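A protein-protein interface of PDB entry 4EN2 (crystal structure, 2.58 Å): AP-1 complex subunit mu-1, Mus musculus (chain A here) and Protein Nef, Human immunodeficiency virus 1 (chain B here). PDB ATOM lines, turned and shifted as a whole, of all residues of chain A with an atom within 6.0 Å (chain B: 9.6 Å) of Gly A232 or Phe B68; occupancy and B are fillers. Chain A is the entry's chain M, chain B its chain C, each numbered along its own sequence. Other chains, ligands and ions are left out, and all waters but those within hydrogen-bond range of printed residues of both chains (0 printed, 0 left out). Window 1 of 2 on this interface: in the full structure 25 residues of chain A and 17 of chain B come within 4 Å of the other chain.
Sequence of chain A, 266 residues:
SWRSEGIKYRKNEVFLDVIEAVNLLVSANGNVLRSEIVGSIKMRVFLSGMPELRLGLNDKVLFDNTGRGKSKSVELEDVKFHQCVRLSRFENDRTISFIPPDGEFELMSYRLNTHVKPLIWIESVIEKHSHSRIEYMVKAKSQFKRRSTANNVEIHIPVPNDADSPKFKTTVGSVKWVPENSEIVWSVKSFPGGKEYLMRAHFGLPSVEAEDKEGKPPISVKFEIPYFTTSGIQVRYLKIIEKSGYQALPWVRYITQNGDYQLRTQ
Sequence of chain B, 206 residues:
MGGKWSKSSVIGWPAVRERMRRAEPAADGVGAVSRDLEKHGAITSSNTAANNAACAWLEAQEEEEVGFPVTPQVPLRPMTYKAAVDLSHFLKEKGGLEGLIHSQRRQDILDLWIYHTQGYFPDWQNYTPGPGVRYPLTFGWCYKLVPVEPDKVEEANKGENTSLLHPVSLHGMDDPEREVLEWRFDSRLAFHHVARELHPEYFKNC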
ATOM      1  N   GLU A  20      -4.717 -13.427   5.736  1.00  0.00           N
ATOM      2  CA  GLU A  20      -3.574 -14.315   5.957  1.00  0.00           C
ATOM      3  C   GLU A  20      -3.764 -15.604   5.208  1.00  0.00           C
ATOM      4  O   GLU A  20      -4.755 -16.302   5.388  1.00  0.00           O
ATOM      5  CB  GLU A  20      -3.358 -14.587   7.438  1.00  0.00           C
ATOM      6  CG  GLU A  20      -3.075 -13.304   8.195  1.00  0.00           C
ATOM      7  CD  GLU A  20      -2.472 -13.508   9.554  1.00  0.00           C
ATOM      8  OE1 GLU A  20      -1.699 -12.613   9.988  1.00  0.00           O
ATOM      9  OE2 GLU A  20      -2.745 -14.574  10.154  1.00  0.00           O
ATOM     10  N   ASN A  58       0.134  -4.631  16.851  1.00  0.00           N
ATOM     11  CA  ASN A  58       0.892  -5.303  17.910  1.00  0.00           C
ATOM     12  C   ASN A  58       2.196  -5.877  17.388  1.00  0.00           C
ATOM     13  O   ASN A  58       2.549  -7.049  17.573  1.00  0.00           O
ATOM     14  CB  ASN A  58       0.067  -6.376  18.591  1.00  0.00           C
ATOM     15  CG  ASN A  58      -0.322  -7.505  17.661  1.00  0.00           C
ATOM     16  OD1 ASN A  58      -0.519  -7.309  16.455  1.00  0.00           O
ATOM     17  ND2 ASN A  58      -0.499  -8.677  18.230  1.00  0.00           N
ATOM     18  N   SER A  73       2.752  -9.735  21.304  1.00  0.00           N
ATOM     19  CA  SER A  73       2.892  -9.120  20.010  1.00  0.00           C
ATOM     20  C   SER A  73       3.067 -10.174  18.930  1.00  0.00           C
ATOM     21  O   SER A  73       2.859 -11.360  19.146  1.00  0.00           O
ATOM     22  CB  SER A  73       4.064  -8.181  20.036  1.00  0.00           C
ATOM     23  OG  SER A  73       5.219  -8.916  20.391  1.00  0.00           O
ATOM     24  N   VAL A  74       3.381  -9.712  17.729  1.00  0.00           N
ATOM     25  CA  VAL A  74       3.604 -10.574  16.595  1.00  0.00           C
ATOM     26  C   VAL A  74       4.868 -10.163  15.907  1.00  0.00           C
ATOM     27  O   VAL A  74       5.084  -8.987  15.609  1.00  0.00           O
ATOM     28  CB  VAL A  74       2.467 -10.439  15.579  1.00  0.00           C
ATOM     29  CG1 VAL A  74       2.832 -11.146  14.288  1.00  0.00           C
ATOM     30  CG2 VAL A  74       1.196 -11.038  16.149  1.00  0.00           C
ATOM     31  N   LYS A 145     -10.315 -23.301  16.470  1.00  0.00           N
ATOM     32  CA  LYS A 145     -11.285 -23.062  17.554  1.00  0.00           C
ATOM     33  C   LYS A 145     -12.711 -23.410  17.176  1.00  0.00           C
ATOM     34  O   LYS A 145     -13.174 -23.024  16.124  1.00  0.00           O
ATOM     35  CB  LYS A 145     -11.260 -21.597  18.012  1.00  0.00           C
ATOM     36  CG  LYS A 145      -9.929 -21.092  18.594  1.00  0.00           C
ATOM     37  CD  LYS A 145      -9.764 -21.423  20.078  1.00  0.00           C
ATOM     38  CE  LYS A 145      -8.381 -21.159  20.646  1.00  0.00           C
ATOM     39  NZ  LYS A 145      -7.552 -20.233  19.836  1.00  0.00           N
ATOM     40  N   SER A 148     -14.999 -20.782  15.680  1.00  0.00           N
ATOM     41  CA  SER A 148     -14.750 -20.450  14.267  1.00  0.00           C
ATOM     42  C   SER A 148     -15.195 -21.517  13.235  1.00  0.00           C
ATOM     43  O   SER A 148     -15.266 -22.718  13.507  1.00  0.00           O
ATOM     44  CB  SER A 148     -13.255 -20.192  14.074  1.00  0.00           C
ATOM     45  OG  SER A 148     -12.773 -19.184  14.935  1.00  0.00           O
ATOM     46  N   TYR A 227     -13.174 -13.898  10.321  1.00  0.00           N
ATOM     47  CA  TYR A 227     -13.196 -13.565  11.755  1.00  0.00           C
ATOM     48  C   TYR A 227     -12.146 -14.297  12.502  1.00  0.00           C
ATOM     49  O   TYR A 227     -12.412 -14.892  13.530  1.00  0.00           O
ATOM     50  CB  TYR A 227     -14.550 -13.884  12.381  1.00  0.00           C
ATOM     51  CG  TYR A 227     -15.651 -13.196  11.656  1.00  0.00           C
ATOM     52  CD1 TYR A 227     -16.603 -13.912  10.939  1.00  0.00           C
ATOM     53  CD2 TYR A 227     -15.691 -11.812  11.603  1.00  0.00           C
ATOM     54  CE1 TYR A 227     -17.604 -13.264  10.240  1.00  0.00           C
ATOM     55  CE2 TYR A 227     -16.677 -11.152  10.890  1.00  0.00           C
ATOM     56  CZ  TYR A 227     -17.628 -11.886  10.216  1.00  0.00           C
ATOM     57  OH  TYR A 227     -18.594 -11.208   9.519  1.00  0.00           O
ATOM     58  N   PHE A 228     -10.935 -14.245  11.994  1.00  0.00           N
ATOM     59  CA  PHE A 228      -9.946 -15.196  12.422  1.00  0.00           C
ATOM     60  C   PHE A 228      -8.589 -14.894  11.849  1.00  0.00           C
ATOM     61  O   PHE A 228      -8.474 -14.646  10.655  1.00  0.00           O
ATOM     62  CB  PHE A 228     -10.375 -16.569  11.918  1.00  0.00           C
ATOM     63  CG  PHE A 228      -9.579 -17.694  12.478  1.00  0.00           C
ATOM     64  CD1 PHE A 228      -9.977 -18.314  13.670  1.00  0.00           C
ATOM     65  CD2 PHE A 228      -8.448 -18.143  11.827  1.00  0.00           C
ATOM     66  CE1 PHE A 228      -9.264 -19.375  14.178  1.00  0.00           C
ATOM     67  CE2 PHE A 228      -7.724 -19.200  12.334  1.00  0.00           C
ATOM     68  CZ  PHE A 228      -8.131 -19.808  13.512  1.00  0.00           C
ATOM     69  N   THR A 229      -7.571 -14.928  12.700  1.00  0.00           N
ATOM     70  CA  THR A 229      -6.167 -14.988  12.250  1.00  0.00           C
ATOM     71  C   THR A 229      -5.382 -16.089  12.915  1.00  0.00           C
ATOM     72  O   THR A 229      -5.671 -16.518  14.013  1.00  0.00           O
ATOM     73  CB  THR A 229      -5.329 -13.704  12.494  1.00  0.00           C
ATOM     74  OG1 THR A 229      -5.145 -13.485  13.895  1.00  0.00           O
ATOM     75  CG2 THR A 229      -5.962 -12.504  11.847  1.00  0.00           C
ATOM     76  N   THR A 230      -4.327 -16.487  12.237  1.00  0.00           N
ATOM     77  CA  THR A 230      -3.419 -17.491  12.728  1.00  0.00           C
ATOM     78  C   THR A 230      -2.328 -16.834  13.523  1.00  0.00           C
ATOM     79  O   THR A 230      -1.963 -17.298  14.594  1.00  0.00           O
ATOM     80  CB  THR A 230      -2.758 -18.163  11.527  1.00  0.00           C
ATOM     81  OG1 THR A 230      -3.757 -18.327  10.512  1.00  0.00           O
ATOM     82  CG2 THR A 230      -2.147 -19.501  11.905  1.00  0.00           C
ATOM     83  N   SER A 231      -1.805 -15.751  12.973  1.00  0.00           N
ATOM     84  CA  SER A 231      -0.653 -15.059  13.534  1.00  0.00           C
ATOM     85  C   SER A 231      -0.959 -14.329  14.808  1.00  0.00           C
ATOM     86  O   SER A 231      -0.058 -14.125  15.639  1.00  0.00           O
ATOM     87  CB  SER A 231      -0.168 -14.030  12.547  1.00  0.00           C
ATOM     88  OG  SER A 231      -1.171 -13.056  12.369  1.00  0.00           O
ATOM     89  N   GLY A 232      -2.219 -13.937  14.961  1.00  0.00           N
ATOM     90  CA  GLY A 232      -2.637 -13.187  16.135  1.00  0.00           C
ATOM     91  C   GLY A 232      -2.336 -11.711  16.004  1.00  0.00           C
ATOM     92  O   GLY A 232      -2.268 -10.956  16.991  1.00  0.00           O
ATOM     93  N   ILE A 233      -2.130 -11.301  14.767  1.00  0.00           N
ATOM     94  CA  ILE A 233      -1.923  -9.902  14.458  1.00  0.00           C
ATOM     95  C   ILE A 233      -3.193  -9.151  14.795  1.00  0.00           C
ATOM     96  O   ILE A 233      -4.297  -9.695  14.661  1.00  0.00           O
ATOM     97  CB  ILE A 233      -1.603  -9.704  12.988  1.00  0.00           C
ATOM     98  CG1 ILE A 233      -1.183  -8.276  12.725  1.00  0.00           C
ATOM     99  CG2 ILE A 233      -2.805 -10.039  12.135  1.00  0.00           C
ATOM    100  CD1 ILE A 233      -0.674  -8.076  11.309  1.00  0.00           C
ATOM    101  N   GLN A 234      -3.012  -7.920  15.281  1.00  0.00           N
ATOM    102  CA  GLN A 234      -4.131  -7.025  15.585  1.00  0.00           C
ATOM    103  C   GLN A 234      -3.802  -5.608  15.141  1.00  0.00           C
ATOM    104  O   GLN A 234      -2.668  -5.137  15.277  1.00  0.00           O
ATOM    105  CB  GLN A 234      -4.526  -7.045  17.069  1.00  0.00           C
ATOM    106  CG  GLN A 234      -3.362  -6.975  18.036  1.00  0.00           C
ATOM    107  CD  GLN A 234      -3.790  -6.724  19.489  1.00  0.00           C
ATOM    108  OE1 GLN A 234      -4.833  -7.213  19.936  1.00  0.00           O
ATOM    109  NE2 GLN A 234      -2.984  -5.949  20.232  1.00  0.00           N
ATOM    110  N   GLU B  62       1.563 -26.997  26.551  1.00  0.00           N
ATOM    111  CA  GLU B  62       0.182 -26.645  26.317  1.00  0.00           C
ATOM    112  C   GLU B  62      -0.208 -26.775  24.853  1.00  0.00           C
ATOM    113  O   GLU B  62       0.580 -26.542  23.933  1.00  0.00           O
ATOM    114  CB  GLU B  62      -0.151 -25.275  26.902  1.00  0.00           C
ATOM    115  CG  GLU B  62       0.168 -24.079  26.029  1.00  0.00           C
ATOM    116  CD  GLU B  62      -1.058 -23.226  25.796  1.00  0.00           C
ATOM    117  OE1 GLU B  62      -0.959 -21.989  25.927  1.00  0.00           O
ATOM    118  OE2 GLU B  62      -2.127 -23.803  25.496  1.00  0.00           O
ATOM    119  N   GLU B  64      -3.000 -26.441  21.528  1.00  0.00           N
ATOM    120  CA  GLU B  64      -3.812 -25.437  20.836  1.00  0.00           C
ATOM    121  C   GLU B  64      -4.997 -26.025  20.055  1.00  0.00           C
ATOM    122  O   GLU B  64      -4.967 -27.141  19.517  1.00  0.00           O
ATOM    123  CB  GLU B  64      -2.961 -24.530  19.891  1.00  0.00           C
ATOM    124  CG  GLU B  64      -2.113 -25.241  18.849  1.00  0.00           C
ATOM    125  CD  GLU B  64      -0.796 -25.768  19.388  1.00  0.00           C
ATOM    126  OE1 GLU B  64      -0.531 -25.646  20.614  1.00  0.00           O
ATOM    127  OE2 GLU B  64      -0.043 -26.329  18.575  1.00  0.00           O
ATOM    128  N   GLU B  65      -6.069 -25.254  20.073  1.00  0.00           N
ATOM    129  CA  GLU B  65      -6.931 -25.162  18.931  1.00  0.00           C
ATOM    130  C   GLU B  65      -6.404 -23.921  18.243  1.00  0.00           C
ATOM    131  O   GLU B  65      -6.500 -22.827  18.785  1.00  0.00           O
ATOM    132  CB  GLU B  65      -8.386 -25.009  19.330  1.00  0.00           C
ATOM    133  CG  GLU B  65      -9.105 -26.334  19.453  1.00  0.00           C
ATOM    134  CD  GLU B  65     -10.605 -26.158  19.404  1.00  0.00           C
ATOM    135  OE1 GLU B  65     -11.089 -25.151  19.959  1.00  0.00           O
ATOM    136  OE2 GLU B  65     -11.292 -27.010  18.801  1.00  0.00           O
ATOM    137  N   VAL B  66      -5.842 -24.104  17.058  1.00  0.00           N
ATOM    138  CA  VAL B  66      -5.054 -23.041  16.387  1.00  0.00           C
ATOM    139  C   VAL B  66      -5.860 -21.778  16.169  1.00  0.00           C
ATOM    140  O   VAL B  66      -7.087 -21.847  15.996  1.00  0.00           O
ATOM    141  CB  VAL B  66      -4.581 -23.429  14.976  1.00  0.00           C
ATOM    142  CG1 VAL B  66      -3.246 -22.788  14.695  1.00  0.00           C
ATOM    143  CG2 VAL B  66      -4.516 -24.933  14.812  1.00  0.00           C
ATOM    144  N   GLY B  67      -5.166 -20.637  16.182  1.00  0.00           N
ATOM    145  CA  GLY B  67      -5.754 -19.359  15.754  1.00  0.00           C
ATOM    146  C   GLY B  67      -6.477 -18.434  16.726  1.00  0.00           C
ATOM    147  O   GLY B  67      -6.782 -18.750  17.871  1.00  0.00           O
ATOM    148  N   PHE B  68      -6.796 -17.265  16.214  1.00  0.00           N
ATOM    149  CA  PHE B  68      -7.233 -16.161  17.042  1.00  0.00           C
ATOM    150  C   PHE B  68      -8.496 -15.645  16.427  1.00  0.00           C
ATOM    151  O   PHE B  68      -8.441 -14.859  15.479  1.00  0.00           O
ATOM    152  CB  PHE B  68      -6.172 -15.060  17.062  1.00  0.00           C
ATOM    153  CG  PHE B  68      -4.890 -15.493  17.664  1.00  0.00           C
ATOM    154  CD1 PHE B  68      -4.653 -15.317  19.001  1.00  0.00           C
ATOM    155  CD2 PHE B  68      -3.929 -16.119  16.888  1.00  0.00           C
ATOM    156  CE1 PHE B  68      -3.469 -15.739  19.568  1.00  0.00           C
ATOM    157  CE2 PHE B  68      -2.731 -16.523  17.445  1.00  0.00           C
ATOM    158  CZ  PHE B  68      -2.506 -16.339  18.790  1.00  0.00           C
ATOM    159  N   PRO B  69      -9.633 -16.100  16.947  1.00  0.00           N
ATOM    160  CA  PRO B  69     -10.907 -15.658  16.443  1.00  0.00           C
ATOM    161  C   PRO B  69     -11.166 -14.261  16.847  1.00  0.00           C
ATOM    162  O   PRO B  69     -10.636 -13.786  17.844  1.00  0.00           O
ATOM    163  CB  PRO B  69     -11.915 -16.565  17.129  1.00  0.00           C
ATOM    164  CG  PRO B  69     -11.183 -17.175  18.247  1.00  0.00           C
ATOM    165  CD  PRO B  69      -9.760 -17.246  17.840  1.00  0.00           C
ATOM    166  N   VAL B  70     -11.986 -13.604  16.064  1.00  0.00           N
ATOM    167  CA  VAL B  70     -12.316 -12.223  16.330  1.00  0.00           C
ATOM    168  C   VAL B  70     -13.830 -12.157  16.392  1.00  0.00           C
ATOM    169  O   VAL B  70     -14.523 -12.558  15.450  1.00  0.00           O
ATOM    170  CB  VAL B  70     -11.789 -11.281  15.241  1.00  0.00           C
ATOM    171  CG1 VAL B  70     -12.730 -10.110  15.054  1.00  0.00           C
ATOM    172  CG2 VAL B  70     -10.401 -10.790  15.589  1.00  0.00           C
ATOM    173  N   THR B  71     -14.353 -11.665  17.502  1.00  0.00           N
ATOM    174  CA  THR B  71     -15.778 -11.692  17.668  1.00  0.00           C
ATOM    175  C   THR B  71     -16.302 -10.579  16.729  1.00  0.00           C
ATOM    176  O   THR B  71     -15.903  -9.427  16.804  1.00  0.00           O
ATOM    177  CB  THR B  71     -16.164 -11.642  19.139  1.00  0.00           C
ATOM    178  OG1 THR B  71     -15.974 -10.328  19.643  1.00  0.00           O
ATOM    179  CG2 THR B  71     -15.290 -12.644  19.952  1.00  0.00           C
ATOM    180  N   PRO B  72     -17.105 -10.968  15.742  1.00  0.00           N
ATOM    181  CA  PRO B  72     -17.415 -10.197  14.528  1.00  0.00           C
ATOM    182  C   PRO B  72     -17.443  -8.667  14.612  1.00  0.00           C
ATOM    183  O   PRO B  72     -16.793  -8.002  13.807  1.00  0.00           O
ATOM    184  CB  PRO B  72     -18.797 -10.740  14.144  1.00  0.00           C
ATOM    185  CG  PRO B  72     -18.746 -12.177  14.553  1.00  0.00           C
ATOM    186  CD  PRO B  72     -17.807 -12.267  15.737  1.00  0.00           C
ATOM    187  N   LEU B  76     -12.350  -3.351  19.697  1.00  0.00           N
ATOM    188  CA  LEU B  76     -11.263  -3.482  20.643  1.00  0.00           C
ATOM    189  C   LEU B  76     -10.324  -2.336  20.440  1.00  0.00           C
ATOM    190  O   LEU B  76      -9.989  -1.959  19.323  1.00  0.00           O
ATOM    191  CB  LEU B  76     -10.531  -4.786  20.387  1.00  0.00           C
ATOM    192  CG  LEU B  76     -11.390  -6.039  20.545  1.00  0.00           C
ATOM    193  CD1 LEU B  76     -10.637  -7.157  19.859  1.00  0.00           C
ATOM    194  CD2 LEU B  76     -11.702  -6.351  22.017  1.00  0.00           C
ATOM    195  N   TYR B 115      -9.703  -6.306  29.810  1.00  0.00           N
ATOM    196  CA  TYR B 115      -9.813  -6.741  28.456  1.00  0.00           C
ATOM    197  C   TYR B 115     -11.163  -7.371  28.177  1.00  0.00           C
ATOM    198  O   TYR B 115     -11.826  -7.009  27.211  1.00  0.00           O
ATOM    199  CB  TYR B 115      -8.742  -7.750  28.146  1.00  0.00           C
ATOM    200  CG  TYR B 115      -8.845  -8.202  26.721  1.00  0.00           C
ATOM    201  CD1 TYR B 115      -8.802  -7.277  25.681  1.00  0.00           C
ATOM    202  CD2 TYR B 115      -9.022  -9.536  26.411  1.00  0.00           C
ATOM    203  CE1 TYR B 115      -8.903  -7.664  24.373  1.00  0.00           C
ATOM    204  CE2 TYR B 115      -9.125  -9.944  25.099  1.00  0.00           C
ATOM    205  CZ  TYR B 115      -9.067  -9.005  24.086  1.00  0.00           C
ATOM    206  OH  TYR B 115      -9.170  -9.423  22.789  1.00  0.00           O
ATOM    207  N   PHE B 121      -7.302  -3.654  24.860  1.00  0.00           N
ATOM    208  CA  PHE B 121      -6.132  -4.470  24.638  1.00  0.00           C
ATOM    209  C   PHE B 121      -5.303  -4.378  25.893  1.00  0.00           C
ATOM    210  O   PHE B 121      -5.030  -3.283  26.364  1.00  0.00           O
ATOM    211  CB  PHE B 121      -5.280  -3.955  23.483  1.00  0.00           C
ATOM    212  CG  PHE B 121      -5.965  -3.966  22.179  1.00  0.00           C
ATOM    213  CD1 PHE B 121      -6.124  -2.803  21.450  1.00  0.00           C
ATOM    214  CD2 PHE B 121      -6.455  -5.155  21.661  1.00  0.00           C
ATOM    215  CE1 PHE B 121      -6.773  -2.819  20.225  1.00  0.00           C
ATOM    216  CE2 PHE B 121      -7.106  -5.171  20.443  1.00  0.00           C
ATOM    217  CZ  PHE B 121      -7.276  -4.004  19.729  1.00  0.00           C
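Lys A145 touches Pro B69 (CG to CD, 3.9 Å).
Ser A148 touches Pro B69 (OG to CB, 3.5 Å).
Tyr A227 touches Pro B69.
Pro B72 touches Tyr A227.
O of Val B66 touches CZ of Phe A228, at 3.4 Å.
CA of Gly B67 touches CZ of Phe A228 (3.3 Å).
Thr A230 touches Phe B68 (O to CE2, 3.1 Å).
C of Ser A231 touches CE2 of Phe B68, at 3.9 Å.
Gly A232 touches Phe B68.
Gln A234 touches Phe B121 (OE1 to CE2, 3.1 Å).
O of Glu B65 is in hydrogen-bond range of NZ of Lys A145 (3.0 Å).
The backbone carbonyl oxygen of Gly B67 lies within hydrogen-bond range of the side-chain amino group of Lys A145.
N of Val B70 sits at hydrogen-bond distance from O of Tyr A227, at 2.9 Å.
O of Thr A229 sits at hydrogen-bond distance from N of Phe B68 (2.6 Å).
Of chain B, only Phe B68 comes within 4 Å of Gly A232.
Of the printed residues of chain A, Phe B68 touches Phe A228 (3.4 Å), Thr A229 (2.6 Å), Thr A230 (3.1 Å), Ser A231 (3.9 Å) and Gly A232 (3.3 Å).
Printed residues of chain B within 4 Å of Thr A229: Gly B67 and Phe B68.
Ser A231 touches one residue of chain B.
Of the printed residues of chain B, Thr A230 touches Phe B68 (3.1 Å).
Of the printed residues of chain A, Pro B72 touches Tyr A227.
Of the printed residues of chain A, Glu B65 touches Lys A145 (3.0 Å).
The nearest residue of chain B that does not touch Gly A232 is Gly B67 (6.4 Å).
OE2 of Glu A20 is in hydrogen-bond range of N of Thr A230 (3.2 Å).
The side-chain carboxylate of Glu A20 is in hydrogen-bond range of the side-chain hydroxyl of Ser A231, 2.5 Å away.
The side-chain amide nitrogen (ND2) of Asn A58 sits at hydrogen-bond distance from the backbone carbonyl oxygen (O) of Gly A232 (3.1 Å).
The side-chain amide oxygen (OD1) of Asn A58 sits at hydrogen-bond distance from the backbone NH (N) of Gln A234, 2.8 Å away.
The side-chain hydroxyl (OG1) of Thr A229 lies within hydrogen-bond range of the backbone NH (N) of Gly A232 (3.1 Å).
N of Ile A233 lies within hydrogen-bond range of OG of Ser A231 (3.1 Å).
Along chain A the printed residues that touch a printed residue of chain B span positions 145 to 234.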
